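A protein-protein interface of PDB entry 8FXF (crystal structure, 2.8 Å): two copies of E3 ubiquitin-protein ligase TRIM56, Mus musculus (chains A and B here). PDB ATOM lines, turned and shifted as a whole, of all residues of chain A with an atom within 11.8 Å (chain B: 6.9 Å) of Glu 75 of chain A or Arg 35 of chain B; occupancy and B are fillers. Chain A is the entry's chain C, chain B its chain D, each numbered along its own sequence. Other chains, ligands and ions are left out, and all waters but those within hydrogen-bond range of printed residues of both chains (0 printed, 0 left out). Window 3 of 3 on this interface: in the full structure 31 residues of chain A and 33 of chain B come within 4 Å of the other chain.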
ATOM      1  N   LEU A  64       4.201  -3.763 -10.766  1.00  0.00           N
ATOM      2  CA  LEU A  64       4.272  -3.912  -9.319  1.00  0.00           C
ATOM      3  C   LEU A  64       4.485  -2.578  -8.617  1.00  0.00           C
ATOM      4  O   LEU A  64       4.065  -2.405  -7.481  1.00  0.00           O
ATOM      5  CB  LEU A  64       5.364  -4.916  -8.923  1.00  0.00           C
ATOM      6  CG  LEU A  64       4.832  -6.328  -8.666  1.00  0.00           C
ATOM      7  CD1 LEU A  64       3.866  -6.735  -9.773  1.00  0.00           C
ATOM      8  CD2 LEU A  64       5.964  -7.336  -8.523  1.00  0.00           C
ATOM      9  N   GLY A  65       5.163  -1.652  -9.286  1.00  0.00           N
ATOM     10  CA  GLY A  65       5.546  -0.423  -8.623  1.00  0.00           C
ATOM     11  C   GLY A  65       4.412   0.586  -8.701  1.00  0.00           C
ATOM     12  O   GLY A  65       4.202   1.349  -7.768  1.00  0.00           O
ATOM     13  N   GLN A  66       3.689   0.571  -9.823  1.00  0.00           N
ATOM     14  CA  GLN A  66       2.556   1.461 -10.006  1.00  0.00           C
ATOM     15  C   GLN A  66       1.348   0.979  -9.172  1.00  0.00           C
ATOM     16  O   GLN A  66       0.573   1.789  -8.668  1.00  0.00           O
ATOM     17  CB  GLN A  66       2.349   1.681 -11.504  1.00  0.00           C
ATOM     18  CG  GLN A  66       1.056   2.395 -11.852  1.00  0.00           C
ATOM     19  CD  GLN A  66       1.070   3.864 -11.510  1.00  0.00           C
ATOM     20  OE1 GLN A  66       0.436   4.290 -10.548  1.00  0.00           O
ATOM     21  NE2 GLN A  66       1.819   4.646 -12.277  1.00  0.00           N
ATOM     22  N   LEU A  67       1.182  -0.337  -8.992  1.00  0.00           N
ATOM     23  CA  LEU A  67       0.255  -0.884  -8.007  1.00  0.00           C
ATOM     24  C   LEU A  67       0.623  -0.466  -6.579  1.00  0.00           C
ATOM     25  O   LEU A  67      -0.259  -0.152  -5.782  1.00  0.00           O
ATOM     26  CB  LEU A  67       0.356  -2.407  -8.055  1.00  0.00           C
ATOM     27  CG  LEU A  67      -0.583  -3.153  -8.988  1.00  0.00           C
ATOM     28  CD1 LEU A  67      -0.399  -4.627  -8.719  1.00  0.00           C
ATOM     29  CD2 LEU A  67      -2.038  -2.734  -8.794  1.00  0.00           C
ATOM     30  N   ARG A  68       1.909  -0.573  -6.209  1.00  0.00           N
ATOM     31  CA  ARG A  68       2.344  -0.167  -4.879  1.00  0.00           C
ATOM     32  C   ARG A  68       1.914   1.282  -4.626  1.00  0.00           C
ATOM     33  O   ARG A  68       1.417   1.606  -3.554  1.00  0.00           O
ATOM     34  CB  ARG A  68       3.858  -0.363  -4.705  1.00  0.00           C
ATOM     35  CG  ARG A  68       4.322  -0.597  -3.269  1.00  0.00           C
ATOM     36  CD  ARG A  68       5.830  -0.674  -3.061  1.00  0.00           C
ATOM     37  NE  ARG A  68       6.506  -1.464  -4.096  1.00  0.00           N
ATOM     38  CZ  ARG A  68       7.490  -1.027  -4.891  1.00  0.00           C
ATOM     39  NH1 ARG A  68       8.081   0.134  -4.646  1.00  0.00           N
ATOM     40  NH2 ARG A  68       7.888  -1.762  -5.924  1.00  0.00           N
ATOM     41  N   ALA A  69       2.076   2.147  -5.637  1.00  0.00           N
ATOM     42  CA  ALA A  69       1.812   3.570  -5.514  1.00  0.00           C
ATOM     43  C   ALA A  69       0.313   3.829  -5.376  1.00  0.00           C
ATOM     44  O   ALA A  69      -0.080   4.816  -4.766  1.00  0.00           O
ATOM     45  CB  ALA A  69       2.412   4.330  -6.676  1.00  0.00           C
ATOM     46  N   LEU A  70      -0.512   2.950  -5.948  1.00  0.00           N
ATOM     47  CA  LEU A  70      -1.964   3.092  -5.924  1.00  0.00           C
ATOM     48  C   LEU A  70      -2.471   2.749  -4.519  1.00  0.00           C
ATOM     49  O   LEU A  70      -3.272   3.503  -3.963  1.00  0.00           O
ATOM     50  CB  LEU A  70      -2.562   2.187  -7.009  1.00  0.00           C
ATOM     51  CG  LEU A  70      -4.077   2.158  -7.187  1.00  0.00           C
ATOM     52  CD1 LEU A  70      -4.415   1.669  -8.594  1.00  0.00           C
ATOM     53  CD2 LEU A  70      -4.765   1.254  -6.169  1.00  0.00           C
ATOM     54  N   VAL A  71      -1.933   1.656  -3.946  1.00  0.00           N
ATOM     55  CA  VAL A  71      -2.190   1.217  -2.584  1.00  0.00           C
ATOM     56  C   VAL A  71      -1.682   2.252  -1.580  1.00  0.00           C
ATOM     57  O   VAL A  71      -2.382   2.559  -0.629  1.00  0.00           O
ATOM     58  CB  VAL A  71      -1.591  -0.175  -2.290  1.00  0.00           C
ATOM     59  CG1 VAL A  71      -1.686  -0.534  -0.813  1.00  0.00           C
ATOM     60  CG2 VAL A  71      -2.208  -1.276  -3.141  1.00  0.00           C
ATOM     61  N   GLU A  72      -0.475   2.789  -1.776  1.00  0.00           N
ATOM     62  CA  GLU A  72       0.070   3.771  -0.841  1.00  0.00           C
ATOM     63  C   GLU A  72      -0.834   5.008  -0.773  1.00  0.00           C
ATOM     64  O   GLU A  72      -1.122   5.503   0.317  1.00  0.00           O
ATOM     65  CB  GLU A  72       1.553   4.077  -1.110  1.00  0.00           C
ATOM     66  CG  GLU A  72       2.445   2.861  -0.860  1.00  0.00           C
ATOM     67  CD  GLU A  72       3.957   3.002  -0.945  1.00  0.00           C
ATOM     68  OE1 GLU A  72       4.456   4.141  -0.967  1.00  0.00           O
ATOM     69  OE2 GLU A  72       4.630   1.960  -1.001  1.00  0.00           O
ATOM     70  N   ALA A  73      -1.304   5.490  -1.933  1.00  0.00           N
ATOM     71  CA  ALA A  73      -2.114   6.698  -1.930  1.00  0.00           C
ATOM     72  C   ALA A  73      -3.455   6.400  -1.258  1.00  0.00           C
ATOM     73  O   ALA A  73      -3.984   7.258  -0.558  1.00  0.00           O
ATOM     74  CB  ALA A  73      -2.288   7.270  -3.332  1.00  0.00           C
ATOM     75  N   ALA A  74      -3.992   5.189  -1.493  1.00  0.00           N
ATOM     76  CA  ALA A  74      -5.270   4.748  -0.945  1.00  0.00           C
ATOM     77  C   ALA A  74      -5.178   4.689   0.575  1.00  0.00           C
ATOM     78  O   ALA A  74      -6.052   5.232   1.248  1.00  0.00           O
ATOM     79  CB  ALA A  74      -5.691   3.410  -1.528  1.00  0.00           C
ATOM     80  N   GLU A  75      -4.109   4.041   1.072  1.00  0.00           N
ATOM     81  CA  GLU A  75      -3.739   3.905   2.473  1.00  0.00           C
ATOM     82  C   GLU A  75      -3.568   5.277   3.126  1.00  0.00           C
ATOM     83  O   GLU A  75      -3.974   5.471   4.267  1.00  0.00           O
ATOM     84  CB  GLU A  75      -2.410   3.160   2.610  1.00  0.00           C
ATOM     85  CG  GLU A  75      -2.531   1.644   2.590  1.00  0.00           C
ATOM     86  CD  GLU A  75      -1.227   0.854   2.569  1.00  0.00           C
ATOM     87  OE1 GLU A  75      -0.145   1.453   2.345  1.00  0.00           O
ATOM     88  OE2 GLU A  75      -1.295  -0.371   2.779  1.00  0.00           O
ATOM     89  N   GLU A  76      -2.945   6.230   2.433  1.00  0.00           N
ATOM     90  CA  GLU A  76      -2.831   7.566   3.013  1.00  0.00           C
ATOM     91  C   GLU A  76      -4.213   8.235   3.108  1.00  0.00           C
ATOM     92  O   GLU A  76      -4.516   8.977   4.040  1.00  0.00           O
ATOM     93  CB  GLU A  76      -1.850   8.438   2.220  1.00  0.00           C
ATOM     94  CG  GLU A  76      -1.558   9.765   2.890  1.00  0.00           C
ATOM     95  CD  GLU A  76      -1.173   9.666   4.362  1.00  0.00           C
ATOM     96  OE1 GLU A  76      -1.755  10.432   5.164  1.00  0.00           O
ATOM     97  OE2 GLU A  76      -0.297   8.815   4.715  1.00  0.00           O
ATOM     98  N   ALA A  77      -5.055   8.008   2.101  1.00  0.00           N
ATOM     99  CA  ALA A  77      -6.360   8.623   2.103  1.00  0.00           C
ATOM    100  C   ALA A  77      -7.133   8.083   3.317  1.00  0.00           C
ATOM    101  O   ALA A  77      -7.451   8.858   4.223  1.00  0.00           O
ATOM    102  CB  ALA A  77      -7.015   8.410   0.753  1.00  0.00           C
ATOM    103  N   THR A  78      -7.309   6.747   3.392  1.00  0.00           N
ATOM    104  CA  THR A  78      -7.895   6.032   4.526  1.00  0.00           C
ATOM    105  C   THR A  78      -7.413   6.555   5.891  1.00  0.00           C
ATOM    106  O   THR A  78      -8.222   6.858   6.765  1.00  0.00           O
ATOM    107  CB  THR A  78      -7.806   4.513   4.331  1.00  0.00           C
ATOM    108  OG1 THR A  78      -8.723   4.224   3.274  1.00  0.00           O
ATOM    109  CG2 THR A  78      -8.201   3.724   5.558  1.00  0.00           C
ATOM    110  N   ARG A  79      -6.101   6.690   6.085  1.00  0.00           N
ATOM    111  CA  ARG A  79      -5.562   7.218   7.325  1.00  0.00           C
ATOM    112  C   ARG A  79      -6.014   8.673   7.561  1.00  0.00           C
ATOM    113  O   ARG A  79      -6.295   9.039   8.700  1.00  0.00           O
ATOM    114  CB  ARG A  79      -4.054   6.950   7.315  1.00  0.00           C
ATOM    115  CG  ARG A  79      -3.274   7.544   8.471  1.00  0.00           C
ATOM    116  CD  ARG A  79      -1.854   7.959   8.104  1.00  0.00           C
ATOM    117  NE  ARG A  79      -1.830   9.354   7.674  1.00  0.00           N
ATOM    118  CZ  ARG A  79      -2.202  10.401   8.418  1.00  0.00           C
ATOM    119  NH1 ARG A  79      -2.176  11.622   7.914  1.00  0.00           N
ATOM    120  NH2 ARG A  79      -2.609  10.234   9.666  1.00  0.00           N
ATOM    121  N   GLU A  80      -6.102   9.507   6.505  1.00  0.00           N
ATOM    122  CA  GLU A  80      -6.624  10.870   6.613  1.00  0.00           C
ATOM    123  C   GLU A  80      -8.097  10.797   7.036  1.00  0.00           C
ATOM    124  O   GLU A  80      -8.618  11.684   7.698  1.00  0.00           O
ATOM    125  CB  GLU A  80      -6.510  11.628   5.280  1.00  0.00           C
ATOM    126  CG  GLU A  80      -5.280  12.520   5.090  1.00  0.00           C
ATOM    127  CD  GLU A  80      -4.807  12.860   3.669  1.00  0.00           C
ATOM    128  OE1 GLU A  80      -5.625  13.280   2.830  1.00  0.00           O
ATOM    129  OE2 GLU A  80      -3.598  12.694   3.377  1.00  0.00           O
ATOM    130  N   ARG A  81      -8.791   9.731   6.633  1.00  0.00           N
ATOM    131  CA  ARG A  81     -10.202   9.586   6.942  1.00  0.00           C
ATOM    132  C   ARG A  81     -10.398   9.305   8.441  1.00  0.00           C
ATOM    133  O   ARG A  81     -11.215   9.948   9.098  1.00  0.00           O
ATOM    134  CB  ARG A  81     -10.824   8.619   5.934  1.00  0.00           C
ATOM    135  CG  ARG A  81     -11.148   9.293   4.609  1.00  0.00           C
ATOM    136  CD  ARG A  81     -11.897   8.527   3.533  1.00  0.00           C
ATOM    137  NE  ARG A  81     -10.857   7.656   3.019  1.00  0.00           N
ATOM    138  CZ  ARG A  81     -10.529   7.578   1.743  1.00  0.00           C
ATOM    139  NH1 ARG A  81     -11.328   8.133   0.852  1.00  0.00           N
ATOM    140  NH2 ARG A  81      -9.471   6.879   1.370  1.00  0.00           N
ATOM    141  N   LEU A  82      -9.579   8.406   8.997  1.00  0.00           N
ATOM    142  CA  LEU A  82      -9.700   7.968  10.380  1.00  0.00           C
ATOM    143  C   LEU A  82      -9.254   9.030  11.387  1.00  0.00           C
ATOM    144  O   LEU A  82      -9.710   9.027  12.528  1.00  0.00           O
ATOM    145  CB  LEU A  82      -8.809   6.743  10.558  1.00  0.00           C
ATOM    146  CG  LEU A  82      -9.052   5.570   9.619  1.00  0.00           C
ATOM    147  CD1 LEU A  82      -8.046   4.470   9.936  1.00  0.00           C
ATOM    148  CD2 LEU A  82     -10.497   5.066   9.688  1.00  0.00           C
ATOM    149  N   THR A  83      -8.299   9.878  10.986  1.00  0.00           N
ATOM    150  CA  THR A  83      -7.804  11.018  11.749  1.00  0.00           C
ATOM    151  C   THR A  83      -8.921  12.045  11.924  1.00  0.00           C
ATOM    152  O   THR A  83      -8.930  12.810  12.891  1.00  0.00           O
ATOM    153  CB  THR A  83      -6.603  11.585  10.981  1.00  0.00           C
ATOM    154  OG1 THR A  83      -5.645  10.537  11.093  1.00  0.00           O
ATOM    155  CG2 THR A  83      -6.041  12.914  11.444  1.00  0.00           C
ATOM    156  N   LYS A  84      -9.847  12.065  10.958  1.00  0.00           N
ATOM    157  CA  LYS A  84     -10.932  13.020  10.962  1.00  0.00           C
ATOM    158  C   LYS A  84     -12.011  12.481  11.896  1.00  0.00           C
ATOM    159  O   LYS A  84     -12.570  13.219  12.700  1.00  0.00           O
ATOM    160  CB  LYS A  84     -11.557  13.110   9.573  1.00  0.00           C
ATOM    161  CG  LYS A  84     -10.971  14.055   8.538  1.00  0.00           C
ATOM    162  CD  LYS A  84     -11.935  14.084   7.338  1.00  0.00           C
ATOM    163  CE  LYS A  84     -12.787  12.821   7.235  1.00  0.00           C
ATOM    164  NZ  LYS A  84     -13.518  12.636   5.952  1.00  0.00           N
ATOM    165  N   LYS B  28     -12.163   0.662   6.819  1.00  0.00           N
ATOM    166  CA  LYS B  28     -11.233  -0.454   6.909  1.00  0.00           C
ATOM    167  C   LYS B  28     -11.648  -1.552   5.916  1.00  0.00           C
ATOM    168  O   LYS B  28     -10.799  -2.064   5.199  1.00  0.00           O
ATOM    169  CB  LYS B  28     -11.159  -0.979   8.340  1.00  0.00           C
ATOM    170  CG  LYS B  28     -10.836   0.031   9.426  1.00  0.00           C
ATOM    171  CD  LYS B  28      -9.384   0.076   9.840  1.00  0.00           C
ATOM    172  CE  LYS B  28      -9.103   0.954  11.047  1.00  0.00           C
ATOM    173  NZ  LYS B  28      -9.028   0.200  12.322  1.00  0.00           N
ATOM    174  N   ALA B  30     -13.044  -1.137   3.192  1.00  0.00           N
ATOM    175  CA  ALA B  30     -12.869  -0.625   1.834  1.00  0.00           C
ATOM    176  C   ALA B  30     -11.413  -0.735   1.390  1.00  0.00           C
ATOM    177  O   ALA B  30     -11.197  -1.061   0.213  1.00  0.00           O
ATOM    178  CB  ALA B  30     -13.385   0.789   1.663  1.00  0.00           C
ATOM    179  N   LEU B  31     -10.480  -0.432   2.328  1.00  0.00           N
ATOM    180  CA  LEU B  31      -9.033  -0.429   2.144  1.00  0.00           C
ATOM    181  C   LEU B  31      -8.487  -1.849   2.138  1.00  0.00           C
ATOM    182  O   LEU B  31      -7.515  -2.118   1.438  1.00  0.00           O
ATOM    183  CB  LEU B  31      -8.333   0.340   3.268  1.00  0.00           C
ATOM    184  CG  LEU B  31      -6.807   0.451   3.096  1.00  0.00           C
ATOM    185  CD1 LEU B  31      -6.395   1.135   1.776  1.00  0.00           C
ATOM    186  CD2 LEU B  31      -6.146   1.164   4.260  1.00  0.00           C
ATOM    187  N   ALA B  32      -9.052  -2.700   3.008  1.00  0.00           N
ATOM    188  CA  ALA B  32      -8.810  -4.134   3.025  1.00  0.00           C
ATOM    189  C   ALA B  32      -9.133  -4.692   1.648  1.00  0.00           C
ATOM    190  O   ALA B  32      -8.261  -5.323   1.050  1.00  0.00           O
ATOM    191  CB  ALA B  32      -9.668  -4.800   4.054  1.00  0.00           C
ATOM    192  N   LEU B  33     -10.356  -4.426   1.145  1.00  0.00           N
ATOM    193  CA  LEU B  33     -10.756  -4.930  -0.168  1.00  0.00           C
ATOM    194  C   LEU B  33      -9.744  -4.448  -1.208  1.00  0.00           C
ATOM    195  O   LEU B  33      -9.315  -5.216  -2.071  1.00  0.00           O
ATOM    196  CB  LEU B  33     -12.187  -4.520  -0.543  1.00  0.00           C
ATOM    197  CG  LEU B  33     -12.696  -5.149  -1.847  1.00  0.00           C
ATOM    198  CD1 LEU B  33     -12.636  -6.671  -1.725  1.00  0.00           C
ATOM    199  CD2 LEU B  33     -14.097  -4.668  -2.288  1.00  0.00           C
ATOM    200  N   LEU B  34      -9.395  -3.157  -1.139  1.00  0.00           N
ATOM    201  CA  LEU B  34      -8.552  -2.579  -2.167  1.00  0.00           C
ATOM    202  C   LEU B  34      -7.192  -3.265  -2.114  1.00  0.00           C
ATOM    203  O   LEU B  34      -6.699  -3.676  -3.155  1.00  0.00           O
ATOM    204  CB  LEU B  34      -8.501  -1.048  -2.023  1.00  0.00           C
ATOM    205  CG  LEU B  34      -7.681  -0.248  -3.045  1.00  0.00           C
ATOM    206  CD1 LEU B  34      -8.101   1.218  -3.048  1.00  0.00           C
ATOM    207  CD2 LEU B  34      -6.181  -0.345  -2.756  1.00  0.00           C
ATOM    208  N   ARG B  35      -6.664  -3.489  -0.903  1.00  0.00           N
ATOM    209  CA  ARG B  35      -5.434  -4.252  -0.700  1.00  0.00           C
ATOM    210  C   ARG B  35      -5.464  -5.669  -1.290  1.00  0.00           C
ATOM    211  O   ARG B  35      -4.458  -6.081  -1.852  1.00  0.00           O
ATOM    212  CB  ARG B  35      -4.946  -4.192   0.750  1.00  0.00           C
ATOM    213  CG  ARG B  35      -4.372  -2.833   1.132  1.00  0.00           C
ATOM    214  CD  ARG B  35      -3.416  -2.868   2.306  1.00  0.00           C
ATOM    215  NE  ARG B  35      -4.190  -2.946   3.531  1.00  0.00           N
ATOM    216  CZ  ARG B  35      -4.023  -2.156   4.587  1.00  0.00           C
ATOM    217  NH1 ARG B  35      -3.050  -1.259   4.597  1.00  0.00           N
ATOM    218  NH2 ARG B  35      -4.809  -2.286   5.645  1.00  0.00           N
ATOM    219  N   GLU B  36      -6.589  -6.391  -1.148  1.00  0.00           N
ATOM    220  CA  GLU B  36      -6.729  -7.716  -1.734  1.00  0.00           C
ATOM    221  C   GLU B  36      -6.584  -7.582  -3.240  1.00  0.00           C
ATOM    222  O   GLU B  36      -5.604  -8.059  -3.803  1.00  0.00           O
ATOM    223  CB  GLU B  36      -8.124  -8.326  -1.563  1.00  0.00           C
ATOM    224  CG  GLU B  36      -8.681  -8.315  -0.155  1.00  0.00           C
ATOM    225  CD  GLU B  36      -8.207  -9.415   0.770  1.00  0.00           C
ATOM    226  OE1 GLU B  36      -7.310 -10.177   0.369  1.00  0.00           O
ATOM    227  OE2 GLU B  36      -8.753  -9.498   1.885  1.00  0.00           O
ATOM    228  N   GLN B  37      -7.577  -6.917  -3.851  1.00  0.00           N
ATOM    229  CA  GLN B  37      -7.682  -6.713  -5.290  1.00  0.00           C
ATOM    230  C   GLN B  37      -6.341  -6.285  -5.923  1.00  0.00           C
ATOM    231  O   GLN B  37      -6.028  -6.634  -7.055  1.00  0.00           O
ATOM    232  CB  GLN B  37      -8.758  -5.649  -5.522  1.00  0.00           C
ATOM    233  CG  GLN B  37     -10.141  -5.941  -4.933  1.00  0.00           C
ATOM    234  CD  GLN B  37     -11.092  -4.783  -5.166  1.00  0.00           C
ATOM    235  OE1 GLN B  37     -10.859  -3.667  -4.688  1.00  0.00           O
ATOM    236  NE2 GLN B  37     -12.150  -5.017  -5.939  1.00  0.00           N
ATOM    237  N   ALA B  38      -5.514  -5.528  -5.201  1.00  0.00           N
ATOM    238  CA  ALA B  38      -4.314  -4.969  -5.791  1.00  0.00           C
ATOM    239  C   ALA B  38      -3.182  -5.989  -5.729  1.00  0.00           C
ATOM    240  O   ALA B  38      -2.538  -6.239  -6.746  1.00  0.00           O
ATOM    241  CB  ALA B  38      -3.951  -3.629  -5.165  1.00  0.00           C
ATOM    242  N   ALA B  39      -2.961  -6.587  -4.550  1.00  0.00           N
ATOM    243  CA  ALA B  39      -1.968  -7.640  -4.353  1.00  0.00           C
ATOM    244  C   ALA B  39      -2.220  -8.809  -5.315  1.00  0.00           C
ATOM    245  O   ALA B  39      -1.289  -9.480  -5.783  1.00  0.00           O
ATOM    246  CB  ALA B  39      -2.006  -8.098  -2.912  1.00  0.00           C
ATOM    247  N   SER B  40      -3.506  -9.009  -5.609  1.00  0.00           N
ATOM    248  CA  SER B  40      -4.031 -10.048  -6.466  1.00  0.00           C
ATOM    249  C   SER B  40      -3.853  -9.726  -7.949  1.00  0.00           C
ATOM    250  O   SER B  40      -3.755 -10.641  -8.753  1.00  0.00           O
ATOM    251  CB  SER B  40      -5.481 -10.261  -6.123  1.00  0.00           C
ATOM    252  OG  SER B  40      -6.174 -10.789  -7.236  1.00  0.00           O
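Leu 67 of chain A touches Ala 38 of chain B (CD1 to O, 3.3 Å).
Val 71 of chain A touches Ala 38 of chain B.
Leu 31 of chain B touches Ala 74 of chain A.
CB of Ala 74 of chain A touches CD1 of Leu 34 of chain B (3.6 Å).
N of Glu 75 of chain A touches CD1 of Leu 31 of chain B, at 3.8 Å.
Leu 31 of chain B touches Thr 78 of chain A.
Lys 28 of chain B touches Leu 82 of chain A (CE to CD1, 3.8 Å).
Hydrophobic or aromatic side chains of chain A within 4 Å of the printed part of chain B: Leu 67, Val 71, Ala 74 and Leu 82.
Along chain A the printed residues that touch a printed residue of chain B span positions 67 to 82.
Among the printed residues, 8 pairs touch across the chains.
Among the printed residues, Asp or Glu carboxylates within 4 Å of a Lys or Arg side-chain nitrogen of the other chain: Glu 75 of chain A with Arg 35 of chain B (2.7 Å).
Of the printed residues of chain B, Val 71 of chain A touches Ala 38.
Printed residues of chain B within 4 Å of Ala 74 of chain A: Leu 31 and Leu 34.
Of chain B, only Leu 31 (3.8 Å) and Arg 35 (2.7 Å) come within 4 Å of Glu 75 of chain A.
Of the printed residues of chain B, Thr 78 of chain A touches Leu 31 (3.5 Å).
Printed residues of chain A within 4 Å of Lys 28 of chain B: Leu 82.
Of the printed residues of chain A, Leu 31 of chain B touches Ala 74, Glu 75 and Thr 78.
No residue of chain A comes within 4 Å of Ala 32 of chain B.
Leu 33 of chain B touches none of the printed residues of chain A.
Leu 34 of chain B touches just one residue of chain A: Ala 74.
Of chain A, only Glu 75 comes within 4 Å of Arg 35 of chain B.
No residue of chain A comes within 4 Å of Gln 37 of chain B.
The nearest printed residue of chain B that does not touch Leu 67 of chain A is Ala 39 of chain B (5.3 Å).
The side-chain carboxylate of Glu 75 of chain A is in salt-bridge range of the guanidinium group of Arg 35 of chain B (2.7 Å).
No position is printed for both chains.
Of the 8 pairs that touch across the chains among the printed residues, none has its exchanged pair printed and touching as well.
The side-chain hydroxyl of Thr 78 of chain A lies within hydrogen-bond range of the guanidinium group of Arg 81 of chain A (3.4 Å).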
